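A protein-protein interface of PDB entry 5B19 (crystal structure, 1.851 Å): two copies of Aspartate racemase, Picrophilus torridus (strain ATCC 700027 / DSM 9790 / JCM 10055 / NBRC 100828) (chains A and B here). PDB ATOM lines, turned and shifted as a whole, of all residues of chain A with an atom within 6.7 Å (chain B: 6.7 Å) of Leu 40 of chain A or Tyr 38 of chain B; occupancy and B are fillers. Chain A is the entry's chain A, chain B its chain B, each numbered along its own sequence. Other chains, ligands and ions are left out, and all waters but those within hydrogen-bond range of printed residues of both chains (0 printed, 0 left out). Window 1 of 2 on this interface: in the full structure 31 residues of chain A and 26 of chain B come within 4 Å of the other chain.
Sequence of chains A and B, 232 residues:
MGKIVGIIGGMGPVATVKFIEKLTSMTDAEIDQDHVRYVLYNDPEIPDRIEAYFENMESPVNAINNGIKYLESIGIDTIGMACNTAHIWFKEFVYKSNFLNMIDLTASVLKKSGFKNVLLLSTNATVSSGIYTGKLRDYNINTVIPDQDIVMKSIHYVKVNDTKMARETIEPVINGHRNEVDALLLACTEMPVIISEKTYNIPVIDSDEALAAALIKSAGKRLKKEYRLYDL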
ATOM      1  N   VAL A   5     -18.877  -3.734 -16.786  1.00  0.00           N
ATOM      2  CA  VAL A   5     -17.520  -4.247 -16.887  1.00  0.00           C
ATOM      3  C   VAL A   5     -17.340  -4.933 -18.240  1.00  0.00           C
ATOM      4  O   VAL A   5     -18.325  -5.212 -18.936  1.00  0.00           O
ATOM      5  CB  VAL A   5     -17.169  -5.225 -15.733  1.00  0.00           C
ATOM      6  CG1 VAL A   5     -17.175  -4.481 -14.391  1.00  0.00           C
ATOM      7  CG2 VAL A   5     -18.125  -6.428 -15.713  1.00  0.00           C
ATOM      8  N   GLY A   6     -16.085  -5.186 -18.611  1.00  0.00           N
ATOM      9  CA  GLY A   6     -15.780  -5.768 -19.913  1.00  0.00           C
ATOM     10  C   GLY A   6     -15.120  -7.129 -19.802  1.00  0.00           C
ATOM     11  O   GLY A   6     -14.285  -7.347 -18.945  1.00  0.00           O
ATOM     12  N   ILE A   7     -15.478  -8.055 -20.679  1.00  0.00           N
ATOM     13  CA  ILE A   7     -14.890  -9.389 -20.590  1.00  0.00           C
ATOM     14  C   ILE A   7     -14.337  -9.785 -21.963  1.00  0.00           C
ATOM     15  O   ILE A   7     -15.021  -9.626 -22.974  1.00  0.00           O
ATOM     16  CB  ILE A   7     -15.922 -10.438 -20.135  1.00  0.00           C
ATOM     17  CG1 ILE A   7     -16.493 -10.089 -18.756  1.00  0.00           C
ATOM     18  CG2 ILE A   7     -15.291 -11.836 -20.126  1.00  0.00           C
ATOM     19  CD1 ILE A   7     -17.674 -10.933 -18.371  1.00  0.00           C
ATOM     20  N   ILE A   8     -13.111 -10.284 -22.006  1.00  0.00           N
ATOM     21  CA  ILE A   8     -12.578 -10.805 -23.268  1.00  0.00           C
ATOM     22  C   ILE A   8     -12.572 -12.323 -23.203  1.00  0.00           C
ATOM     23  O   ILE A   8     -12.018 -12.923 -22.285  1.00  0.00           O
ATOM     24  CB  ILE A   8     -11.185 -10.262 -23.560  1.00  0.00           C
ATOM     25  CG1 ILE A   8     -11.269  -8.737 -23.654  1.00  0.00           C
ATOM     26  CG2 ILE A   8     -10.641 -10.828 -24.885  1.00  0.00           C
ATOM     27  CD1 ILE A   8      -9.961  -8.038 -23.831  1.00  0.00           C
ATOM     28  N   GLY A   9     -13.229 -12.936 -24.176  1.00  0.00           N
ATOM     29  CA  GLY A   9     -13.402 -14.370 -24.169  1.00  0.00           C
ATOM     30  C   GLY A   9     -13.186 -14.939 -25.551  1.00  0.00           C
ATOM     31  O   GLY A   9     -12.694 -14.229 -26.439  1.00  0.00           O
ATOM     32  N   GLY A  10     -13.557 -16.207 -25.719  1.00  0.00           N
ATOM     33  CA  GLY A  10     -13.373 -16.933 -26.968  1.00  0.00           C
ATOM     34  C   GLY A  10     -12.200 -17.896 -26.938  1.00  0.00           C
ATOM     35  O   GLY A  10     -11.792 -18.468 -27.961  1.00  0.00           O
ATOM     36  N   PRO A  13     -14.350 -20.985 -26.697  1.00  0.00           N
ATOM     37  CA  PRO A  13     -15.787 -20.720 -26.616  1.00  0.00           C
ATOM     38  C   PRO A  13     -16.509 -21.581 -25.574  1.00  0.00           C
ATOM     39  O   PRO A  13     -17.341 -21.059 -24.831  1.00  0.00           O
ATOM     40  CB  PRO A  13     -16.281 -21.051 -28.026  1.00  0.00           C
ATOM     41  CG  PRO A  13     -15.124 -20.878 -28.882  1.00  0.00           C
ATOM     42  CD  PRO A  13     -13.945 -21.351 -28.067  1.00  0.00           C
ATOM     43  N   THR A  16     -15.669 -20.278 -22.256  1.00  0.00           N
ATOM     44  CA  THR A  16     -16.186 -18.932 -22.030  1.00  0.00           C
ATOM     45  C   THR A  16     -17.635 -18.970 -21.529  1.00  0.00           C
ATOM     46  O   THR A  16     -18.004 -18.226 -20.629  1.00  0.00           O
ATOM     47  CB  THR A  16     -16.108 -18.067 -23.314  1.00  0.00           C
ATOM     48  OG1 THR A  16     -14.757 -18.033 -23.785  1.00  0.00           O
ATOM     49  CG2 THR A  16     -16.568 -16.641 -23.022  1.00  0.00           C
ATOM     50  N   VAL A  17     -18.433 -19.857 -22.106  1.00  0.00           N
ATOM     51  CA  VAL A  17     -19.806 -20.071 -21.660  1.00  0.00           C
ATOM     52  C   VAL A  17     -19.832 -20.453 -20.187  1.00  0.00           C
ATOM     53  O   VAL A  17     -20.594 -19.900 -19.403  1.00  0.00           O
ATOM     54  CB  VAL A  17     -20.498 -21.174 -22.472  1.00  0.00           C
ATOM     55  CG1 VAL A  17     -21.860 -21.500 -21.853  1.00  0.00           C
ATOM     56  CG2 VAL A  17     -20.641 -20.740 -23.943  1.00  0.00           C
ATOM     57  N   PHE A  19     -17.453 -19.819 -18.077  1.00  0.00           N
ATOM     58  CA  PHE A  19     -17.009 -18.655 -17.313  1.00  0.00           C
ATOM     59  C   PHE A  19     -18.181 -17.712 -17.003  1.00  0.00           C
ATOM     60  O   PHE A  19     -18.362 -17.270 -15.866  1.00  0.00           O
ATOM     61  CB  PHE A  19     -15.902 -17.876 -18.049  1.00  0.00           C
ATOM     62  CG  PHE A  19     -15.463 -16.641 -17.304  1.00  0.00           C
ATOM     63  CD1 PHE A  19     -14.566 -16.745 -16.246  1.00  0.00           C
ATOM     64  CD2 PHE A  19     -15.979 -15.395 -17.621  1.00  0.00           C
ATOM     65  CE1 PHE A  19     -14.176 -15.627 -15.525  1.00  0.00           C
ATOM     66  CE2 PHE A  19     -15.587 -14.267 -16.914  1.00  0.00           C
ATOM     67  CZ  PHE A  19     -14.674 -14.383 -15.863  1.00  0.00           C
ATOM     68  N   ILE A  20     -18.981 -17.401 -18.015  1.00  0.00           N
ATOM     69  CA  ILE A  20     -20.108 -16.496 -17.826  1.00  0.00           C
ATOM     70  C   ILE A  20     -21.169 -17.080 -16.866  1.00  0.00           C
ATOM     71  O   ILE A  20     -21.763 -16.365 -16.056  1.00  0.00           O
ATOM     72  CB  ILE A  20     -20.763 -16.164 -19.170  1.00  0.00           C
ATOM     73  CG1 ILE A  20     -19.765 -15.464 -20.098  1.00  0.00           C
ATOM     74  CG2 ILE A  20     -21.998 -15.320 -18.959  1.00  0.00           C
ATOM     75  CD1 ILE A  20     -19.334 -14.105 -19.585  1.00  0.00           C
ATOM     76  N   TYR A  38     -22.429  -6.373 -18.233  1.00  0.00           N
ATOM     77  CA  TYR A  38     -21.139  -6.523 -18.906  1.00  0.00           C
ATOM     78  C   TYR A  38     -21.283  -6.544 -20.425  1.00  0.00           C
ATOM     79  O   TYR A  38     -22.370  -6.784 -20.961  1.00  0.00           O
ATOM     80  CB  TYR A  38     -20.423  -7.798 -18.415  1.00  0.00           C
ATOM     81  CG  TYR A  38     -21.133  -9.093 -18.722  1.00  0.00           C
ATOM     82  CD1 TYR A  38     -20.947  -9.737 -19.941  1.00  0.00           C
ATOM     83  CD2 TYR A  38     -21.985  -9.679 -17.801  1.00  0.00           C
ATOM     84  CE1 TYR A  38     -21.602 -10.940 -20.233  1.00  0.00           C
ATOM     85  CE2 TYR A  38     -22.643 -10.880 -18.086  1.00  0.00           C
ATOM     86  CZ  TYR A  38     -22.446 -11.497 -19.299  1.00  0.00           C
ATOM     87  OH  TYR A  38     -23.103 -12.672 -19.580  1.00  0.00           O
ATOM     88  N   VAL A  39     -20.168  -6.273 -21.099  1.00  0.00           N
ATOM     89  CA  VAL A  39     -20.030  -6.477 -22.530  1.00  0.00           C
ATOM     90  C   VAL A  39     -18.976  -7.558 -22.713  1.00  0.00           C
ATOM     91  O   VAL A  39     -17.842  -7.404 -22.246  1.00  0.00           O
ATOM     92  CB  VAL A  39     -19.627  -5.178 -23.260  1.00  0.00           C
ATOM     93  CG1 VAL A  39     -19.349  -5.443 -24.749  1.00  0.00           C
ATOM     94  CG2 VAL A  39     -20.723  -4.137 -23.100  1.00  0.00           C
ATOM     95  N   LEU A  40     -19.374  -8.670 -23.320  1.00  0.00           N
ATOM     96  CA  LEU A  40     -18.450  -9.766 -23.605  1.00  0.00           C
ATOM     97  C   LEU A  40     -17.941  -9.682 -25.034  1.00  0.00           C
ATOM     98  O   LEU A  40     -18.717  -9.811 -25.984  1.00  0.00           O
ATOM     99  CB  LEU A  40     -19.128 -11.121 -23.387  1.00  0.00           C
ATOM    100  CG  LEU A  40     -18.413 -12.375 -23.897  1.00  0.00           C
ATOM    101  CD1 LEU A  40     -17.067 -12.612 -23.212  1.00  0.00           C
ATOM    102  CD2 LEU A  40     -19.319 -13.598 -23.758  1.00  0.00           C
ATOM    103  N   TYR A  41     -16.642  -9.466 -25.185  1.00  0.00           N
ATOM    104  CA  TYR A  41     -16.010  -9.500 -26.497  1.00  0.00           C
ATOM    105  C   TYR A  41     -15.497 -10.911 -26.737  1.00  0.00           C
ATOM    106  O   TYR A  41     -14.436 -11.284 -26.244  1.00  0.00           O
ATOM    107  CB  TYR A  41     -14.882  -8.488 -26.567  1.00  0.00           C
ATOM    108  CG  TYR A  41     -14.285  -8.304 -27.939  1.00  0.00           C
ATOM    109  CD1 TYR A  41     -14.756  -7.308 -28.792  1.00  0.00           C
ATOM    110  CD2 TYR A  41     -13.229  -9.096 -28.368  1.00  0.00           C
ATOM    111  CE1 TYR A  41     -14.191  -7.121 -30.052  1.00  0.00           C
ATOM    112  CE2 TYR A  41     -12.662  -8.927 -29.624  1.00  0.00           C
ATOM    113  CZ  TYR A  41     -13.142  -7.941 -30.460  1.00  0.00           C
ATOM    114  OH  TYR A  41     -12.568  -7.768 -31.705  1.00  0.00           O
ATOM    115  N   ASN A  42     -16.276 -11.700 -27.468  1.00  0.00           N
ATOM    116  CA  ASN A  42     -16.023 -13.120 -27.608  1.00  0.00           C
ATOM    117  C   ASN A  42     -15.442 -13.387 -28.978  1.00  0.00           C
ATOM    118  O   ASN A  42     -16.183 -13.508 -29.948  1.00  0.00           O
ATOM    119  CB  ASN A  42     -17.330 -13.909 -27.391  1.00  0.00           C
ATOM    120  CG  ASN A  42     -17.127 -15.420 -27.364  1.00  0.00           C
ATOM    121  OD1 ASN A  42     -16.467 -15.985 -28.219  1.00  0.00           O
ATOM    122  ND2 ASN A  42     -17.739 -16.081 -26.387  1.00  0.00           N
ATOM    123  N   ASP A  43     -14.110 -13.429 -29.066  1.00  0.00           N
ATOM    124  CA  ASP A  43     -13.433 -13.589 -30.346  1.00  0.00           C
ATOM    125  C   ASP A  43     -12.650 -14.894 -30.411  1.00  0.00           C
ATOM    126  O   ASP A  43     -11.460 -14.927 -30.127  1.00  0.00           O
ATOM    127  CB  ASP A  43     -12.493 -12.401 -30.610  1.00  0.00           C
ATOM    128  CG  ASP A  43     -11.957 -12.387 -32.028  1.00  0.00           C
ATOM    129  OD1 ASP A  43     -12.258 -13.340 -32.786  1.00  0.00           O
ATOM    130  OD2 ASP A  43     -11.219 -11.430 -32.382  1.00  0.00           O
ATOM    131  N   PRO A  44     -13.311 -15.979 -30.839  1.00  0.00           N
ATOM    132  CA  PRO A  44     -12.585 -17.248 -30.911  1.00  0.00           C
ATOM    133  C   PRO A  44     -11.576 -17.316 -32.055  1.00  0.00           C
ATOM    134  O   PRO A  44     -10.816 -18.274 -32.104  1.00  0.00           O
ATOM    135  CB  PRO A  44     -13.700 -18.286 -31.106  1.00  0.00           C
ATOM    136  CG  PRO A  44     -14.866 -17.517 -31.641  1.00  0.00           C
ATOM    137  CD  PRO A  44     -14.758 -16.130 -31.089  1.00  0.00           C
ATOM    138  N   LEU A  71     -14.008  -2.400 -26.089  1.00  0.00           N
ATOM    139  CA  LEU A  71     -14.588  -2.309 -24.759  1.00  0.00           C
ATOM    140  C   LEU A  71     -14.399  -0.918 -24.153  1.00  0.00           C
ATOM    141  O   LEU A  71     -15.340  -0.340 -23.613  1.00  0.00           O
ATOM    142  CB  LEU A  71     -13.988  -3.375 -23.844  1.00  0.00           C
ATOM    143  CG  LEU A  71     -14.322  -4.820 -24.229  1.00  0.00           C
ATOM    144  CD1 LEU A  71     -13.615  -5.822 -23.328  1.00  0.00           C
ATOM    145  CD2 LEU A  71     -15.817  -5.062 -24.220  1.00  0.00           C
ATOM    146  N   LYS B   3     -17.397 -12.719 -39.776  1.00  0.00           N
ATOM    147  CA  LYS B   3     -17.791 -11.389 -39.327  1.00  0.00           C
ATOM    148  C   LYS B   3     -18.198 -11.451 -37.858  1.00  0.00           C
ATOM    149  O   LYS B   3     -18.844 -12.407 -37.440  1.00  0.00           O
ATOM    150  CB  LYS B   3     -18.953 -10.860 -40.172  1.00  0.00           C
ATOM    151  CG  LYS B   3     -18.629 -10.705 -41.656  1.00  0.00           C
ATOM    152  CD  LYS B   3     -19.752  -9.976 -42.399  1.00  0.00           C
ATOM    153  CE  LYS B   3     -20.341 -10.845 -43.508  1.00  0.00           C
ATOM    154  NZ  LYS B   3     -20.983 -12.084 -42.950  1.00  0.00           N
ATOM    155  N   ILE B   4     -17.819 -10.445 -37.084  1.00  0.00           N
ATOM    156  CA  ILE B   4     -18.318 -10.320 -35.722  1.00  0.00           C
ATOM    157  C   ILE B   4     -19.801  -9.972 -35.796  1.00  0.00           C
ATOM    158  O   ILE B   4     -20.199  -9.127 -36.593  1.00  0.00           O
ATOM    159  CB  ILE B   4     -17.572  -9.249 -34.945  1.00  0.00           C
ATOM    160  CG1 ILE B   4     -16.070  -9.544 -34.953  1.00  0.00           C
ATOM    161  CG2 ILE B   4     -18.094  -9.148 -33.495  1.00  0.00           C
ATOM    162  CD1 ILE B   4     -15.243  -8.375 -34.510  1.00  0.00           C
ATOM    163  N   VAL B   5     -20.612 -10.638 -34.982  1.00  0.00           N
ATOM    164  CA  VAL B   5     -22.029 -10.311 -34.869  1.00  0.00           C
ATOM    165  C   VAL B   5     -22.332  -9.787 -33.469  1.00  0.00           C
ATOM    166  O   VAL B   5     -21.512  -9.909 -32.565  1.00  0.00           O
ATOM    167  CB  VAL B   5     -22.911 -11.521 -35.171  1.00  0.00           C
ATOM    168  CG1 VAL B   5     -22.708 -11.955 -36.613  1.00  0.00           C
ATOM    169  CG2 VAL B   5     -22.575 -12.657 -34.223  1.00  0.00           C
ATOM    170  N   GLY B   6     -23.517  -9.213 -33.295  1.00  0.00           N
ATOM    171  CA  GLY B   6     -23.876  -8.566 -32.049  1.00  0.00           C
ATOM    172  C   GLY B   6     -25.013  -9.273 -31.342  1.00  0.00           C
ATOM    173  O   GLY B   6     -25.954  -9.760 -31.969  1.00  0.00           O
ATOM    174  N   ILE B   7     -24.914  -9.362 -30.025  1.00  0.00           N
ATOM    175  CA  ILE B   7     -26.002  -9.931 -29.251  1.00  0.00           C
ATOM    176  C   ILE B   7     -26.352  -9.021 -28.089  1.00  0.00           C
ATOM    177  O   ILE B   7     -25.475  -8.544 -27.376  1.00  0.00           O
ATOM    178  CB  ILE B   7     -25.649 -11.339 -28.730  1.00  0.00           C
ATOM    179  CG1 ILE B   7     -25.252 -12.234 -29.900  1.00  0.00           C
ATOM    180  CG2 ILE B   7     -26.839 -11.940 -28.008  1.00  0.00           C
ATOM    181  CD1 ILE B   7     -24.556 -13.514 -29.477  1.00  0.00           C
ATOM    182  N   ILE B  20     -26.252 -18.348 -25.127  1.00  0.00           N
ATOM    183  CA  ILE B  20     -24.915 -18.411 -25.690  1.00  0.00           C
ATOM    184  C   ILE B  20     -24.361 -19.832 -25.655  1.00  0.00           C
ATOM    185  O   ILE B  20     -23.541 -20.204 -26.492  1.00  0.00           O
ATOM    186  CB  ILE B  20     -23.941 -17.431 -24.999  1.00  0.00           C
ATOM    187  CG1 ILE B  20     -23.735 -17.749 -23.519  1.00  0.00           C
ATOM    188  CG2 ILE B  20     -24.447 -16.004 -25.162  1.00  0.00           C
ATOM    189  CD1 ILE B  20     -22.591 -16.926 -22.905  1.00  0.00           C
ATOM    190  N   GLU B  21     -24.805 -20.635 -24.704  1.00  0.00           N
ATOM    191  CA  GLU B  21     -24.418 -22.035 -24.710  1.00  0.00           C
ATOM    192  C   GLU B  21     -25.011 -22.725 -25.938  1.00  0.00           C
ATOM    193  O   GLU B  21     -24.354 -23.563 -26.577  1.00  0.00           O
ATOM    194  CB  GLU B  21     -24.870 -22.718 -23.422  1.00  0.00           C
ATOM    195  CG  GLU B  21     -24.481 -24.170 -23.329  1.00  0.00           C
ATOM    196  CD  GLU B  21     -25.007 -24.813 -22.071  1.00  0.00           C
ATOM    197  OE1 GLU B  21     -26.208 -25.157 -22.043  1.00  0.00           O
ATOM    198  OE2 GLU B  21     -24.224 -24.967 -21.107  1.00  0.00           O
ATOM    199  N   LEU B  23     -25.840 -21.310 -28.828  1.00  0.00           N
ATOM    200  CA  LEU B  23     -25.067 -20.800 -29.948  1.00  0.00           C
ATOM    201  C   LEU B  23     -23.783 -21.597 -30.154  1.00  0.00           C
ATOM    202  O   LEU B  23     -23.458 -21.999 -31.270  1.00  0.00           O
ATOM    203  CB  LEU B  23     -24.720 -19.326 -29.735  1.00  0.00           C
ATOM    204  CG  LEU B  23     -23.944 -18.726 -30.907  1.00  0.00           C
ATOM    205  CD1 LEU B  23     -24.898 -18.518 -32.042  1.00  0.00           C
ATOM    206  CD2 LEU B  23     -23.298 -17.411 -30.508  1.00  0.00           C
ATOM    207  N   THR B  24     -23.058 -21.815 -29.067  1.00  0.00           N
ATOM    208  CA  THR B  24     -21.812 -22.565 -29.131  1.00  0.00           C
ATOM    209  C   THR B  24     -22.042 -24.013 -29.531  1.00  0.00           C
ATOM    210  O   THR B  24     -21.307 -24.569 -30.332  1.00  0.00           O
ATOM    211  CB  THR B  24     -21.074 -22.549 -27.787  1.00  0.00           C
ATOM    212  OG1 THR B  24     -20.956 -21.197 -27.334  1.00  0.00           O
ATOM    213  CG2 THR B  24     -19.685 -23.150 -27.934  1.00  0.00           C
ATOM    214  N   VAL B  36     -18.164 -18.813 -33.552  1.00  0.00           N
ATOM    215  CA  VAL B  36     -18.748 -17.523 -33.896  1.00  0.00           C
ATOM    216  C   VAL B  36     -18.123 -16.403 -33.098  1.00  0.00           C
ATOM    217  O   VAL B  36     -17.996 -16.499 -31.877  1.00  0.00           O
ATOM    218  CB  VAL B  36     -20.262 -17.535 -33.659  1.00  0.00           C
ATOM    219  CG1 VAL B  36     -20.844 -16.125 -33.788  1.00  0.00           C
ATOM    220  CG2 VAL B  36     -20.924 -18.492 -34.636  1.00  0.00           C
ATOM    221  N   ARG B  37     -17.730 -15.346 -33.801  1.00  0.00           N
ATOM    222  CA  ARG B  37     -17.250 -14.143 -33.161  1.00  0.00           C
ATOM    223  C   ARG B  37     -18.429 -13.248 -32.824  1.00  0.00           C
ATOM    224  O   ARG B  37     -19.208 -12.890 -33.716  1.00  0.00           O
ATOM    225  CB  ARG B  37     -16.281 -13.397 -34.068  1.00  0.00           C
ATOM    226  CG  ARG B  37     -15.195 -14.278 -34.650  1.00  0.00           C
ATOM    227  CD  ARG B  37     -14.429 -13.502 -35.698  1.00  0.00           C
ATOM    228  NE  ARG B  37     -13.419 -12.627 -35.104  1.00  0.00           N
ATOM    229  CZ  ARG B  37     -13.019 -11.476 -35.638  1.00  0.00           C
ATOM    230  NH1 ARG B  37     -13.558 -11.050 -36.782  1.00  0.00           N
ATOM    231  NH2 ARG B  37     -12.089 -10.744 -35.031  1.00  0.00           N
ATOM    232  N   TYR B  38     -18.566 -12.874 -31.555  1.00  0.00           N
ATOM    233  CA  TYR B  38     -19.625 -11.934 -31.215  1.00  0.00           C
ATOM    234  C   TYR B  38     -19.266 -11.006 -30.069  1.00  0.00           C
ATOM    235  O   TYR B  38     -18.318 -11.234 -29.308  1.00  0.00           O
ATOM    236  CB  TYR B  38     -20.924 -12.666 -30.870  1.00  0.00           C
ATOM    237  CG  TYR B  38     -20.846 -13.561 -29.655  1.00  0.00           C
ATOM    238  CD1 TYR B  38     -21.095 -13.062 -28.378  1.00  0.00           C
ATOM    239  CD2 TYR B  38     -20.531 -14.900 -29.782  1.00  0.00           C
ATOM    240  CE1 TYR B  38     -21.027 -13.886 -27.260  1.00  0.00           C
ATOM    241  CE2 TYR B  38     -20.465 -15.729 -28.677  1.00  0.00           C
ATOM    242  CZ  TYR B  38     -20.712 -15.218 -27.418  1.00  0.00           C
ATOM    243  OH  TYR B  38     -20.644 -16.038 -26.305  1.00  0.00           O
ATOM    244  N   VAL B  39     -20.046  -9.941 -29.984  1.00  0.00           N
ATOM    245  CA  VAL B  39     -20.008  -9.059 -28.847  1.00  0.00           C
ATOM    246  C   VAL B  39     -21.376  -9.128 -28.218  1.00  0.00           C
ATOM    247  O   VAL B  39     -22.382  -8.862 -28.877  1.00  0.00           O
ATOM    248  CB  VAL B  39     -19.663  -7.632 -29.241  1.00  0.00           C
ATOM    249  CG1 VAL B  39     -19.696  -6.757 -28.016  1.00  0.00           C
ATOM    250  CG2 VAL B  39     -18.288  -7.589 -29.907  1.00  0.00           C
ATOM    251  N   LEU B  40     -21.403  -9.543 -26.958  1.00  0.00           N
ATOM    252  CA  LEU B  40     -22.636  -9.686 -26.209  1.00  0.00           C
ATOM    253  C   LEU B  40     -22.794  -8.502 -25.266  1.00  0.00           C
ATOM    254  O   LEU B  40     -21.929  -8.252 -24.434  1.00  0.00           O
ATOM    255  CB  LEU B  40     -22.628 -10.991 -25.426  1.00  0.00           C
ATOM    256  CG  LEU B  40     -23.637 -11.096 -24.279  1.00  0.00           C
ATOM    257  CD1 LEU B  40     -25.072 -10.961 -24.785  1.00  0.00           C
ATOM    258  CD2 LEU B  40     -23.428 -12.414 -23.523  1.00  0.00           C
ATOM    259  N   TYR B  41     -23.879  -7.750 -25.419  1.00  0.00           N
ATOM    260  CA  TYR B  41     -24.144  -6.650 -24.500  1.00  0.00           C
ATOM    261  C   TYR B  41     -25.196  -7.122 -23.530  1.00  0.00           C
ATOM    262  O   TYR B  41     -26.359  -7.291 -23.880  1.00  0.00           O
ATOM    263  CB  TYR B  41     -24.587  -5.392 -25.244  1.00  0.00           C
ATOM    264  CG  TYR B  41     -25.307  -4.385 -24.385  1.00  0.00           C
ATOM    265  CD1 TYR B  41     -24.703  -3.812 -23.271  1.00  0.00           C
ATOM    266  CD2 TYR B  41     -26.588  -3.986 -24.706  1.00  0.00           C
ATOM    267  CE1 TYR B  41     -25.383  -2.876 -22.492  1.00  0.00           C
ATOM    268  CE2 TYR B  41     -27.261  -3.058 -23.952  1.00  0.00           C
ATOM    269  CZ  TYR B  41     -26.664  -2.504 -22.851  1.00  0.00           C
ATOM    270  OH  TYR B  41     -27.377  -1.577 -22.115  1.00  0.00           O
ATOM    271  N   ASN B  42     -24.760  -7.390 -22.308  1.00  0.00           N
ATOM    272  CA  ASN B  42     -25.625  -8.009 -21.315  1.00  0.00           C
ATOM    273  C   ASN B  42     -26.005  -6.988 -20.242  1.00  0.00           C
ATOM    274  O   ASN B  42     -25.178  -6.627 -19.400  1.00  0.00           O
ATOM    275  CB  ASN B  42     -24.925  -9.233 -20.698  1.00  0.00           C
ATOM    276  CG  ASN B  42     -25.838 -10.033 -19.783  1.00  0.00           C
ATOM    277  OD1 ASN B  42     -26.379 -11.068 -20.172  1.00  0.00           O
ATOM    278  ND2 ASN B  42     -26.014  -9.556 -18.568  1.00  0.00           N
ATOM    279  N   ILE B  76     -20.360  -3.985 -36.505  1.00  0.00           N
ATOM    280  CA  ILE B  76     -21.260  -5.127 -36.579  1.00  0.00           C
ATOM    281  C   ILE B  76     -22.459  -4.878 -37.510  1.00  0.00           C
ATOM    282  O   ILE B  76     -23.086  -3.822 -37.462  1.00  0.00           O
ATOM    283  CB  ILE B  76     -21.746  -5.500 -35.163  1.00  0.00           C
ATOM    284  CG1 ILE B  76     -20.565  -6.028 -34.336  1.00  0.00           C
ATOM    285  CG2 ILE B  76     -22.836  -6.548 -35.220  1.00  0.00           C
ATOM    286  CD1 ILE B  76     -20.871  -6.170 -32.845  1.00  0.00           C
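Among the printed residues, merely in contact across the chains: Val 17 of chain A with Ile 20 of chain B (3.9 Å), Val 17 of chain A with Glu 21 of chain B (3.6 Å), Val 17 of chain A with Thr 24 of chain B (3.4 Å), Tyr 38 of chain A with Leu 40 of chain B (3.8 Å), Tyr 38 of chain A with Tyr 41 of chain B (3.8 Å), Val 39 of chain A with Val 39 of chain B (3.5 Å), Val 39 of chain A with Leu 40 of chain B (3.2 Å), Val 39 of chain A with Tyr 41 of chain B (3.997 Å), Leu 40 of chain A with Tyr 38 of chain B (3.6 Å), Leu 40 of chain A with Val 39 of chain B (3.2 Å), Tyr 41 of chain A with Ile 4 of chain B (3.9 Å), Tyr 41 of chain A with Tyr 38 of chain B (3.8 Å), Tyr 41 of chain A with Val 39 of chain B (3.7 Å), Asn 42 of chain A with Val 36 of chain B (3.99 Å), Asn 42 of chain A with Arg 37 of chain B (3.4 Å), Pro 44 of chain A with Val 36 of chain B (3.3 Å) and Pro 44 of chain A with Arg 37 of chain B (3.8 Å).
O of Tyr 38 of chain A lies within hydrogen-bond range of N of Asn 42 of chain B, at 2.8 Å. The backbone NH (N) of Leu 40 of chain A is in hydrogen-bond range of the backbone carbonyl oxygen (O) of Leu 40 of chain B, at 2.8 Å. The backbone NH of Asn 42 of chain A lies within hydrogen-bond range of the backbone carbonyl oxygen of Tyr 38 of chain B (2.8 Å). The guanidinium group (NE) of Arg 37 of chain B is in salt-bridge range of the side-chain carboxylate (OD1) of Asp 43 of chain A (2.7 Å).
O of Val 39 of chain A sits at hydrogen-bond distance from N of Ile 7 of chain A, at 2.9 Å. The backbone carbonyl oxygen (O) of Ile 7 of chain A lies within hydrogen-bond range of the backbone NH (N) of Tyr 41 of chain A, 2.7 Å away. O of Tyr 41 of chain A is in hydrogen-bond range of N of Gly 9 of chain A (2.9 Å). The backbone carbonyl oxygen (O) of Arg 37 of chain B sits at hydrogen-bond distance from the backbone NH (N) of Val 5 of chain B, 2.9 Å away. The backbone NH (N) of Val 39 of chain B is in hydrogen-bond range of the backbone carbonyl oxygen (O) of Val 5 of chain B (3.0 Å). OG1 of Thr 24 of chain B sits at hydrogen-bond distance from O of Ile 20 of chain B, 2.9 Å away.
Tyr 38 of chain A touches Tyr 41 of chain B, and with the chains exchanged Tyr 41 of chain A touches Tyr 38 of chain B. Tyr 38 of chain A touches Asn 42 of chain B, and with the chains exchanged Asn 42 of chain A touches Tyr 38 of chain B. Val 39 of chain B touches its own counterpart, Val 39 of chain A. Leu 40 of chain B touches its own counterpart, Leu 40 of chain A. 9 positions are printed for both chains. Of the 21 pairs that touch across the chains among the printed residues, 12 have their exchanged pair printed and touching as well.
Hydrophobic or aromatic side chains of chain B that line the printed part of chain A: Ile 4, Tyr 38, Val 39, Leu 40 and Tyr 41. Along chain B the printed residues that touch a printed residue of chain A span positions 4 to 42. Hydrophobic or aromatic side chains of chain A within 4 Å of the printed part of chain B: Val 17, Tyr 38, Val 39, Leu 40, Tyr 41 and Pro 44. Among the printed residues, 21 pairs touch across the chains. Among the printed residues, Asp or Glu carboxylates within 4 Å of a Lys or Arg side-chain nitrogen of the other chain: Asp 43 of chain A with Arg 37 of chain B.
Of the printed residues of chain B, Tyr 38 of chain A touches Leu 40 (3.8 Å), Tyr 41 (3.8 Å) and Asn 42 (2.8 Å). Of the printed residues of chain B, Leu 40 of chain A touches Tyr 38, Val 39 and Leu 40. Leu 23 of chain B touches none of the printed residues of chain A. Of the printed residues of chain A, Val 36 of chain B touches Asn 42 (3.99 Å) and Pro 44 (3.3 Å). Tyr 38 of chain B touches three residues of chain A. The nearest residue of chain B that does not touch Leu 40 of chain A is Ile 20 of chain B (4.7 Å). The nearest residue of chain A that does not touch Tyr 38 of chain B is Asp 43 of chain A (4.8 Å).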
